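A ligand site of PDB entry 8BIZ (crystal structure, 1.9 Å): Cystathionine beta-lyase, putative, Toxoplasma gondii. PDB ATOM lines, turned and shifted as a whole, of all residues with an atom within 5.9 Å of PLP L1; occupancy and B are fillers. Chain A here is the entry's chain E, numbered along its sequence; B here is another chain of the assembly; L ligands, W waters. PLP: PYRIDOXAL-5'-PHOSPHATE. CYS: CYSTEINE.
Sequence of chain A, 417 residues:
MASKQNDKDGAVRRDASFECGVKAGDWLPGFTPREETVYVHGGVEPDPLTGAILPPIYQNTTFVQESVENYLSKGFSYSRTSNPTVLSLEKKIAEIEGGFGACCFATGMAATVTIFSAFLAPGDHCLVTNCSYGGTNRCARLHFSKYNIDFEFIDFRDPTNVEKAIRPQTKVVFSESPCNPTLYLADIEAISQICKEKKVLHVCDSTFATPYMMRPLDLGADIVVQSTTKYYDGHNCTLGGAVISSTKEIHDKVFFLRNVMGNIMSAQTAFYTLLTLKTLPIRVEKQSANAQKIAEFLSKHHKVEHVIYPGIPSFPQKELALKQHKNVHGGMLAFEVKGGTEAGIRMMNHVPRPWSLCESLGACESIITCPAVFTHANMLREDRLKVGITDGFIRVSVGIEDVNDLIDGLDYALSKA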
ATOM      1  N   THR A 107      25.821   4.074  26.511  1.00  0.00           N
ATOM      2  CA  THR A 107      24.746   3.420  25.769  1.00  0.00           C
ATOM      3  C   THR A 107      23.672   4.428  25.364  1.00  0.00           C
ATOM      4  O   THR A 107      23.594   5.532  25.911  1.00  0.00           O
ATOM      5  CB  THR A 107      24.055   2.305  26.587  1.00  0.00           C
ATOM      6  OG1 THR A 107      23.413   2.886  27.733  1.00  0.00           O
ATOM      7  CG2 THR A 107      25.026   1.179  27.032  1.00  0.00           C
ATOM      8  N   GLY A 108      22.812   4.020  24.427  1.00  0.00           N
ATOM      9  CA  GLY A 108      21.609   4.787  24.147  1.00  0.00           C
ATOM     10  C   GLY A 108      20.717   4.955  25.367  1.00  0.00           C
ATOM     11  O   GLY A 108      20.179   6.040  25.611  1.00  0.00           O
ATOM     12  N   MET A 109      20.555   3.885  26.154  1.00  0.00           N
ATOM     13  CA  MET A 109      19.729   3.994  27.362  1.00  0.00           C
ATOM     14  C   MET A 109      20.308   5.014  28.341  1.00  0.00           C
ATOM     15  O   MET A 109      19.561   5.695  29.042  1.00  0.00           O
ATOM     16  CB  MET A 109      19.600   2.624  28.051  1.00  0.00           C
ATOM     17  CG  MET A 109      18.583   1.671  27.392  1.00  0.00           C
ATOM     18  SD  MET A 109      16.941   2.399  27.141  1.00  0.00           S
ATOM     19  CE  MET A 109      16.560   2.922  28.813  1.00  0.00           C
ATOM     20  N   ALA A 110      21.634   5.114  28.422  1.00  0.00           N
ATOM     21  CA  ALA A 110      22.234   6.129  29.297  1.00  0.00           C
ATOM     22  C   ALA A 110      21.894   7.540  28.815  1.00  0.00           C
ATOM     23  O   ALA A 110      21.609   8.431  29.627  1.00  0.00           O
ATOM     24  CB  ALA A 110      23.749   5.936  29.367  1.00  0.00           C
ATOM     25  N   THR A 112      19.147   8.393  27.175  1.00  0.00           N
ATOM     26  CA  THR A 112      17.724   8.584  27.481  1.00  0.00           C
ATOM     27  C   THR A 112      17.507   8.856  28.967  1.00  0.00           C
ATOM     28  O   THR A 112      16.764   9.773  29.344  1.00  0.00           O
ATOM     29  CB  THR A 112      16.920   7.347  27.064  1.00  0.00           C
ATOM     30  OG1 THR A 112      17.092   7.119  25.656  1.00  0.00           O
ATOM     31  CG2 THR A 112      15.437   7.501  27.420  1.00  0.00           C
ATOM     32  N   TYR A 133      10.477   2.496  22.063  1.00  0.00           N
ATOM     33  CA  TYR A 133      11.375   1.375  22.305  1.00  0.00           C
ATOM     34  C   TYR A 133      11.161   0.864  23.726  1.00  0.00           C
ATOM     35  O   TYR A 133      11.024   1.661  24.662  1.00  0.00           O
ATOM     36  CB  TYR A 133      12.830   1.802  22.078  1.00  0.00           C
ATOM     37  CG  TYR A 133      13.878   0.878  22.626  1.00  0.00           C
ATOM     38  CD1 TYR A 133      14.635   1.221  23.747  1.00  0.00           C
ATOM     39  CD2 TYR A 133      14.140  -0.347  22.016  1.00  0.00           C
ATOM     40  CE1 TYR A 133      15.604   0.358  24.245  1.00  0.00           C
ATOM     41  CE2 TYR A 133      15.108  -1.199  22.504  1.00  0.00           C
ATOM     42  CZ  TYR A 133      15.827  -0.842  23.614  1.00  0.00           C
ATOM     43  OH  TYR A 133      16.781  -1.701  24.086  1.00  0.00           O
ATOM     44  N   THR A 136      12.964   2.374  26.803  1.00  0.00           N
ATOM     45  CA  THR A 136      12.509   3.715  27.179  1.00  0.00           C
ATOM     46  C   THR A 136      11.233   3.623  28.005  1.00  0.00           C
ATOM     47  O   THR A 136      11.137   4.199  29.103  1.00  0.00           O
ATOM     48  CB  THR A 136      12.269   4.538  25.918  1.00  0.00           C
ATOM     49  OG1 THR A 136      13.434   4.501  25.087  1.00  0.00           O
ATOM     50  CG2 THR A 136      11.918   5.986  26.266  1.00  0.00           C
ATOM     51  N   GLU A 176       9.449   9.356  19.011  1.00  0.00           N
ATOM     52  CA  GLU A 176      10.354   8.410  18.367  1.00  0.00           C
ATOM     53  C   GLU A 176       9.833   8.191  16.950  1.00  0.00           C
ATOM     54  O   GLU A 176       8.621   8.039  16.764  1.00  0.00           O
ATOM     55  CB  GLU A 176      10.414   7.100  19.157  1.00  0.00           C
ATOM     56  CG  GLU A 176      11.379   6.032  18.657  1.00  0.00           C
ATOM     57  CD  GLU A 176      11.304   4.756  19.469  1.00  0.00           C
ATOM     58  OE1 GLU A 176      11.207   4.856  20.724  1.00  0.00           O
ATOM     59  OE2 GLU A 176      11.302   3.650  18.896  1.00  0.00           O
ATOM     60  N   PRO A 178      11.233   6.564  12.923  1.00  0.00           N
ATOM     61  CA  PRO A 178      10.167   5.555  13.077  1.00  0.00           C
ATOM     62  C   PRO A 178      10.254   4.866  14.443  1.00  0.00           C
ATOM     63  O   PRO A 178      11.355   4.752  14.983  1.00  0.00           O
ATOM     64  CB  PRO A 178      10.444   4.559  11.942  1.00  0.00           C
ATOM     65  CG  PRO A 178      11.304   5.315  10.963  1.00  0.00           C
ATOM     66  CD  PRO A 178      12.120   6.262  11.789  1.00  0.00           C
ATOM     67  N   ASN A 180      10.129   1.878  17.310  1.00  0.00           N
ATOM     68  CA  ASN A 180      10.543   0.492  17.467  1.00  0.00           C
ATOM     69  C   ASN A 180       9.443  -0.283  18.172  1.00  0.00           C
ATOM     70  O   ASN A 180       9.051   0.088  19.285  1.00  0.00           O
ATOM     71  CB  ASN A 180      11.815   0.426  18.312  1.00  0.00           C
ATOM     72  CG  ASN A 180      12.482  -0.943  18.298  1.00  0.00           C
ATOM     73  OD1 ASN A 180      11.854  -1.964  17.991  1.00  0.00           O
ATOM     74  ND2 ASN A 180      13.763  -0.969  18.661  1.00  0.00           N
ATOM     75  N   ASP A 205      13.798  10.614  19.680  1.00  0.00           N
ATOM     76  CA  ASP A 205      14.663   9.453  19.451  1.00  0.00           C
ATOM     77  C   ASP A 205      14.574   9.089  17.982  1.00  0.00           C
ATOM     78  O   ASP A 205      13.610   8.464  17.540  1.00  0.00           O
ATOM     79  CB  ASP A 205      14.242   8.277  20.342  1.00  0.00           C
ATOM     80  CG  ASP A 205      15.205   7.086  20.251  1.00  0.00           C
ATOM     81  OD1 ASP A 205      15.948   6.937  19.244  1.00  0.00           O
ATOM     82  OD2 ASP A 205      15.184   6.250  21.181  1.00  0.00           O
ATOM     83  N   THR A 207      16.813   7.123  16.366  1.00  0.00           N
ATOM     84  CA  THR A 207      17.741   6.011  16.122  1.00  0.00           C
ATOM     85  C   THR A 207      17.404   5.262  14.833  1.00  0.00           C
ATOM     86  O   THR A 207      18.309   4.934  14.053  1.00  0.00           O
ATOM     87  CB  THR A 207      17.738   5.043  17.298  1.00  0.00           C
ATOM     88  OG1 THR A 207      18.263   5.676  18.466  1.00  0.00           O
ATOM     89  CG2 THR A 207      18.550   3.789  16.969  1.00  0.00           C
ATOM     90  N   PHE A 208      16.130   4.950  14.621  1.00  0.00           N
ATOM     91  CA  PHE A 208      15.741   4.153  13.445  1.00  0.00           C
ATOM     92  C   PHE A 208      15.913   4.937  12.147  1.00  0.00           C
ATOM     93  O   PHE A 208      16.030   4.334  11.080  1.00  0.00           O
ATOM     94  CB  PHE A 208      14.293   3.685  13.571  1.00  0.00           C
ATOM     95  CG  PHE A 208      14.135   2.356  14.224  1.00  0.00           C
ATOM     96  CD1 PHE A 208      14.891   2.007  15.332  1.00  0.00           C
ATOM     97  CD2 PHE A 208      13.175   1.458  13.761  1.00  0.00           C
ATOM     98  CE1 PHE A 208      14.715   0.769  15.952  1.00  0.00           C
ATOM     99  CE2 PHE A 208      12.994   0.221  14.373  1.00  0.00           C
ATOM    100  CZ  PHE A 208      13.769  -0.115  15.461  1.00  0.00           C
ATOM    101  N   VAL A 225      17.971  12.227  20.744  1.00  0.00           N
ATOM    102  CA  VAL A 225      18.612  11.096  21.391  1.00  0.00           C
ATOM    103  C   VAL A 225      18.951  10.078  20.311  1.00  0.00           C
ATOM    104  O   VAL A 225      18.140   9.825  19.405  1.00  0.00           O
ATOM    105  CB  VAL A 225      17.692  10.489  22.471  1.00  0.00           C
ATOM    106  CG1 VAL A 225      18.166   9.107  22.885  1.00  0.00           C
ATOM    107  CG2 VAL A 225      17.624  11.406  23.676  1.00  0.00           C
ATOM    108  N   SER A 227      20.723   6.079  19.882  1.00  0.00           N
ATOM    109  CA  SER A 227      21.556   4.926  20.224  1.00  0.00           C
ATOM    110  C   SER A 227      22.578   4.788  19.111  1.00  0.00           C
ATOM    111  O   SER A 227      22.270   4.351  17.992  1.00  0.00           O
ATOM    112  CB  SER A 227      20.724   3.661  20.372  1.00  0.00           C
ATOM    113  OG  SER A 227      21.578   2.529  20.511  1.00  0.00           O
ATOM    114  N   THR A 228      23.826   5.181  19.407  1.00  0.00           N
ATOM    115  CA  THR A 228      24.868   5.008  18.392  1.00  0.00           C
ATOM    116  C   THR A 228      25.213   3.539  18.171  1.00  0.00           C
ATOM    117  O   THR A 228      25.835   3.211  17.157  1.00  0.00           O
ATOM    118  CB  THR A 228      26.136   5.798  18.761  1.00  0.00           C
ATOM    119  OG1 THR A 228      26.741   5.244  19.932  1.00  0.00           O
ATOM    120  CG2 THR A 228      25.814   7.260  19.002  1.00  0.00           C
ATOM    121  N   THR A 229      24.792   2.657  19.096  1.00  0.00           N
ATOM    122  CA  THR A 229      24.948   1.203  18.947  1.00  0.00           C
ATOM    123  C   THR A 229      24.470   0.711  17.591  1.00  0.00           C
ATOM    124  O   THR A 229      25.054  -0.210  17.000  1.00  0.00           O
ATOM    125  CB  THR A 229      24.140   0.509  20.045  1.00  0.00           C
ATOM    126  OG1 THR A 229      24.466   1.078  21.323  1.00  0.00           O
ATOM    127  CG2 THR A 229      24.399  -0.998  20.038  1.00  0.00           C
ATOM    128  N   LYS A 230      23.399   1.311  17.075  1.00  0.00           N
ATOM    129  CA  LYS A 230      22.657   0.716  15.975  1.00  0.00           C
ATOM    130  C   LYS A 230      23.291   1.074  14.633  1.00  0.00           C
ATOM    131  O   LYS A 230      24.067   0.284  14.095  1.00  0.00           O
ATOM    132  CB  LYS A 230      21.191   1.168  16.044  1.00  0.00           C
ATOM    133  CG  LYS A 230      20.546   0.901  17.406  1.00  0.00           C
ATOM    134  CD  LYS A 230      20.749  -0.532  17.845  1.00  0.00           C
ATOM    135  CE  LYS A 230      20.356  -0.752  19.317  1.00  0.00           C
ATOM    136  NZ  LYS A 230      18.964  -0.294  19.601  1.00  0.00           N
ATOM    137  N   LEU A 239      28.705  -0.502  21.995  1.00  0.00           N
ATOM    138  CA  LEU A 239      27.541   0.163  22.543  1.00  0.00           C
ATOM    139  C   LEU A 239      27.811   1.661  22.660  1.00  0.00           C
ATOM    140  O   LEU A 239      28.936   2.090  22.913  1.00  0.00           O
ATOM    141  CB  LEU A 239      27.204  -0.375  23.946  1.00  0.00           C
ATOM    142  CG  LEU A 239      26.924  -1.858  24.148  1.00  0.00           C
ATOM    143  CD1 LEU A 239      26.916  -2.156  25.627  1.00  0.00           C
ATOM    144  CD2 LEU A 239      25.606  -2.223  23.515  1.00  0.00           C
ATOM    145  N   GLY A 240      26.767   2.457  22.494  1.00  0.00           N
ATOM    146  CA  GLY A 240      26.948   3.877  22.705  1.00  0.00           C
ATOM    147  C   GLY A 240      25.674   4.684  22.609  1.00  0.00           C
ATOM    148  O   GLY A 240      24.680   4.214  22.047  1.00  0.00           O
ATOM    149  N   GLY A 241      25.708   5.914  23.126  1.00  0.00           N
ATOM    150  CA  GLY A 241      24.569   6.797  23.048  1.00  0.00           C
ATOM    151  C   GLY A 241      25.015   8.232  22.805  1.00  0.00           C
ATOM    152  O   GLY A 241      26.170   8.594  23.032  1.00  0.00           O
ATOM    153  N   LEU A 361      19.922  -4.055  15.878  1.00  0.00           N
ATOM    154  CA  LEU A 361      19.519  -3.637  14.541  1.00  0.00           C
ATOM    155  C   LEU A 361      20.552  -2.650  14.022  1.00  0.00           C
ATOM    156  O   LEU A 361      21.402  -2.154  14.759  1.00  0.00           O
ATOM    157  CB  LEU A 361      18.126  -3.012  14.563  1.00  0.00           C
ATOM    158  CG  LEU A 361      18.009  -1.781  15.485  1.00  0.00           C
ATOM    159  CD1 LEU A 361      17.956  -0.460  14.739  1.00  0.00           C
ATOM    160  CD2 LEU A 361      16.839  -1.929  16.440  1.00  0.00           C
ATOM    161  N   TYR B  78      22.580  -9.410  24.796  1.00  0.00           N
ATOM    162  CA  TYR B  78      22.870  -8.026  24.459  1.00  0.00           C
ATOM    163  C   TYR B  78      23.856  -7.437  25.470  1.00  0.00           C
ATOM    164  O   TYR B  78      23.654  -7.567  26.678  1.00  0.00           O
ATOM    165  CB  TYR B  78      21.581  -7.197  24.443  1.00  0.00           C
ATOM    166  CG  TYR B  78      21.664  -5.850  23.776  1.00  0.00           C
ATOM    167  CD1 TYR B  78      21.900  -5.733  22.409  1.00  0.00           C
ATOM    168  CD2 TYR B  78      21.483  -4.681  24.517  1.00  0.00           C
ATOM    169  CE1 TYR B  78      21.954  -4.500  21.798  1.00  0.00           C
ATOM    170  CE2 TYR B  78      21.541  -3.439  23.905  1.00  0.00           C
ATOM    171  CZ  TYR B  78      21.775  -3.342  22.548  1.00  0.00           C
ATOM    172  OH  TYR B  78      21.845  -2.116  21.927  1.00  0.00           O
ATOM    173  N   ARG B  80      24.594  -4.528  26.595  1.00  0.00           N
ATOM    174  CA  ARG B  80      24.169  -3.587  27.631  1.00  0.00           C
ATOM    175  C   ARG B  80      23.700  -4.332  28.868  1.00  0.00           C
ATOM    176  O   ARG B  80      23.851  -3.842  30.001  1.00  0.00           O
ATOM    177  CB  ARG B  80      23.049  -2.654  27.124  1.00  0.00           C
ATOM    178  CG  ARG B  80      22.317  -1.949  28.280  1.00  0.00           C
ATOM    179  CD  ARG B  80      21.510  -0.709  27.937  1.00  0.00           C
ATOM    180  NE  ARG B  80      20.729  -0.833  26.701  1.00  0.00           N
ATOM    181  CZ  ARG B  80      19.660  -1.591  26.550  1.00  0.00           C
ATOM    182  NH1 ARG B  80      19.223  -2.365  27.535  1.00  0.00           N
ATOM    183  NH2 ARG B  80      19.018  -1.606  25.380  1.00  0.00           N
ATOM    184  N   GLY B 262      21.770   1.762  31.608  1.00  0.00           N
ATOM    185  CA  GLY B 262      22.706   1.701  30.484  1.00  0.00           C
ATOM    186  C   GLY B 262      24.116   2.140  30.825  1.00  0.00           C
ATOM    187  O   GLY B 262      24.778   2.747  29.978  1.00  0.00           O
HETATM  188  N1  PLP L   1      16.070   3.743  21.298  1.00  0.00           N
HETATM  189  C2  PLP L   1      15.949   2.941  20.193  1.00  0.00           C
HETATM  190  C2A PLP L   1      14.990   3.350  19.101  1.00  0.00           C
HETATM  191  C3  PLP L   1      16.693   1.773  20.098  1.00  0.00           C
HETATM  192  O3  PLP L   1      16.602   0.960  19.009  1.00  0.00           O
HETATM  193  C4  PLP L   1      17.578   1.420  21.112  1.00  0.00           C
HETATM  194  C4A PLP L   1      18.528   0.297  20.830  1.00  0.00           C
HETATM  195  C5  PLP L   1      17.688   2.239  22.248  1.00  0.00           C
HETATM  196  C6  PLP L   1      16.939   3.398  22.321  1.00  0.00           C
HETATM  197  C5A PLP L   1      18.612   1.880  23.389  1.00  0.00           C
HETATM  198  O4P PLP L   1      19.983   2.031  23.061  1.00  0.00           O
HETATM  199  P   PLP L   1      21.105   1.062  23.700  1.00  0.00           P
HETATM  200  O1P PLP L   1      21.154   1.239  25.197  1.00  0.00           O
HETATM  201  O2P PLP L   1      20.732  -0.364  23.385  1.00  0.00           O
HETATM  202  O3P PLP L   1      22.411   1.466  23.044  1.00  0.00           O
HETATM  203  N   CYS L   2      18.105  -2.729  20.826  1.00  0.00           N
HETATM  204  CA  CYS L   2      17.786  -4.063  21.245  1.00  0.00           C
HETATM  205  C   CYS L   2      16.569  -4.524  20.438  1.00  0.00           C
HETATM  206  O   CYS L   2      15.780  -3.657  19.946  1.00  0.00           O
HETATM  207  CB  CYS L   2      17.569  -4.081  22.755  1.00  0.00           C
HETATM  208  SG  CYS L   2      17.869  -5.756  23.402  1.00  0.00           S
HETATM  209  OXT CYS L   2      16.349  -5.744  20.244  1.00  0.00           O
HETATM  210  O   HOH W   1      16.024   4.815  25.151  1.00  0.00           O
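A carbon (C4A) of PLP L1 is bonded to the side-chain amino group (NZ) of Lys 230, 1.4 Å away. An oxygen (O2P) of PLP L1 is in hydrogen-bond range of the side-chain hydroxyl (OH) of Tyr 78 of chain B. The guanidinium group (NE) of Arg 80 of chain B lies within salt-bridge range of an oxygen (O1P) of PLP L1, at 2.6 Å. The side-chain carboxylate of Asp 205 is in hydrogen-bond range of a nitrogen (N1) of PLP L1 (2.7 Å). O3P of PLP L1 lies within hydrogen-bond range of OG1 of Thr 229 (2.7 Å). The side-chain hydroxyl of Ser 227 is in hydrogen-bond range of an oxygen (O3P) of PLP L1, 2.9 Å away. The backbone NH (N) of Met 109 sits at hydrogen-bond distance from an oxygen (O1P) of PLP L1 (2.9 Å). N of Gly 108 sits at hydrogen-bond distance from O3P of PLP L1. An oxygen (O3) of PLP L1 lies within hydrogen-bond range of the side-chain amide nitrogen of Asn 180. NZ of Lys 230 lies close to N of CYS L2, at 2.9 Å.
The side-chain hydroxyl (OH) of Tyr 133 lies within hydrogen-bond range of the guanidinium group (NH2) of Arg 80 of chain B (2.6 Å). OG1 of Thr 207 sits at hydrogen-bond distance from OD1 of Asp 205 (2.7 Å). OG of Ser 227 lies close to OG1 of Thr 229, 3.3 Å away. The backbone NH (N) of Gly 240 is in hydrogen-bond range of the side-chain hydroxyl (OG1) of Thr 229 (2.9 Å). The backbone NH (N) of Gly 108 is in hydrogen-bond range of the backbone carbonyl oxygen (O) of Gly 240 (3.0 Å). The side-chain hydroxyl of Thr 107 sits at hydrogen-bond distance from the backbone carbonyl oxygen of Gly 262 of chain B (2.6 Å). The backbone NH (N) of Tyr 133 lies within hydrogen-bond range of the side-chain carboxylate (OE1) of Glu 176. The backbone NH of Thr 228 sits at hydrogen-bond distance from the backbone carbonyl oxygen of Gly 240, 2.9 Å away.
Thr 107 touches PLP L1. Tyr 133 touches PLP L1 (CE1 to C5, 3.4 Å). Glu 176 touches PLP L1. Thr 207 touches PLP L1 (CB to C2A, 3.7 Å). Phe 208 touches PLP L1. O of Gly 240 touches O3P of PLP L1, 3.7 Å away. Leu 361 touches PLP L1 (CD2 to O3, 3.9 Å). Hydrophobic or aromatic side chains within 4 Å of PLP L1: Met 109, Tyr 133, Phe 208, Leu 361 and Tyr 78 of chain B. Within 4 Å of PLP L1: Thr 107, Gly 108, Met 109, Tyr 133, Glu 176, Asn 180, Asp 205, Thr 207, Phe 208, Ser 227, Thr 229, Lys 230, Gly 240, Leu 361, Tyr 78 of chain B and Arg 80 of chain B. The nearest printed residue that does not touch PLP L1 is Thr 136 (4.6 Å).
Water W1 lies within hydrogen-bond range of the side-chain hydroxyl of Thr 112 (2.6 Å), the side-chain hydroxyl of Thr 136 (2.6 Å) and the side-chain sulfur of Met 109 (3.3 Å).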
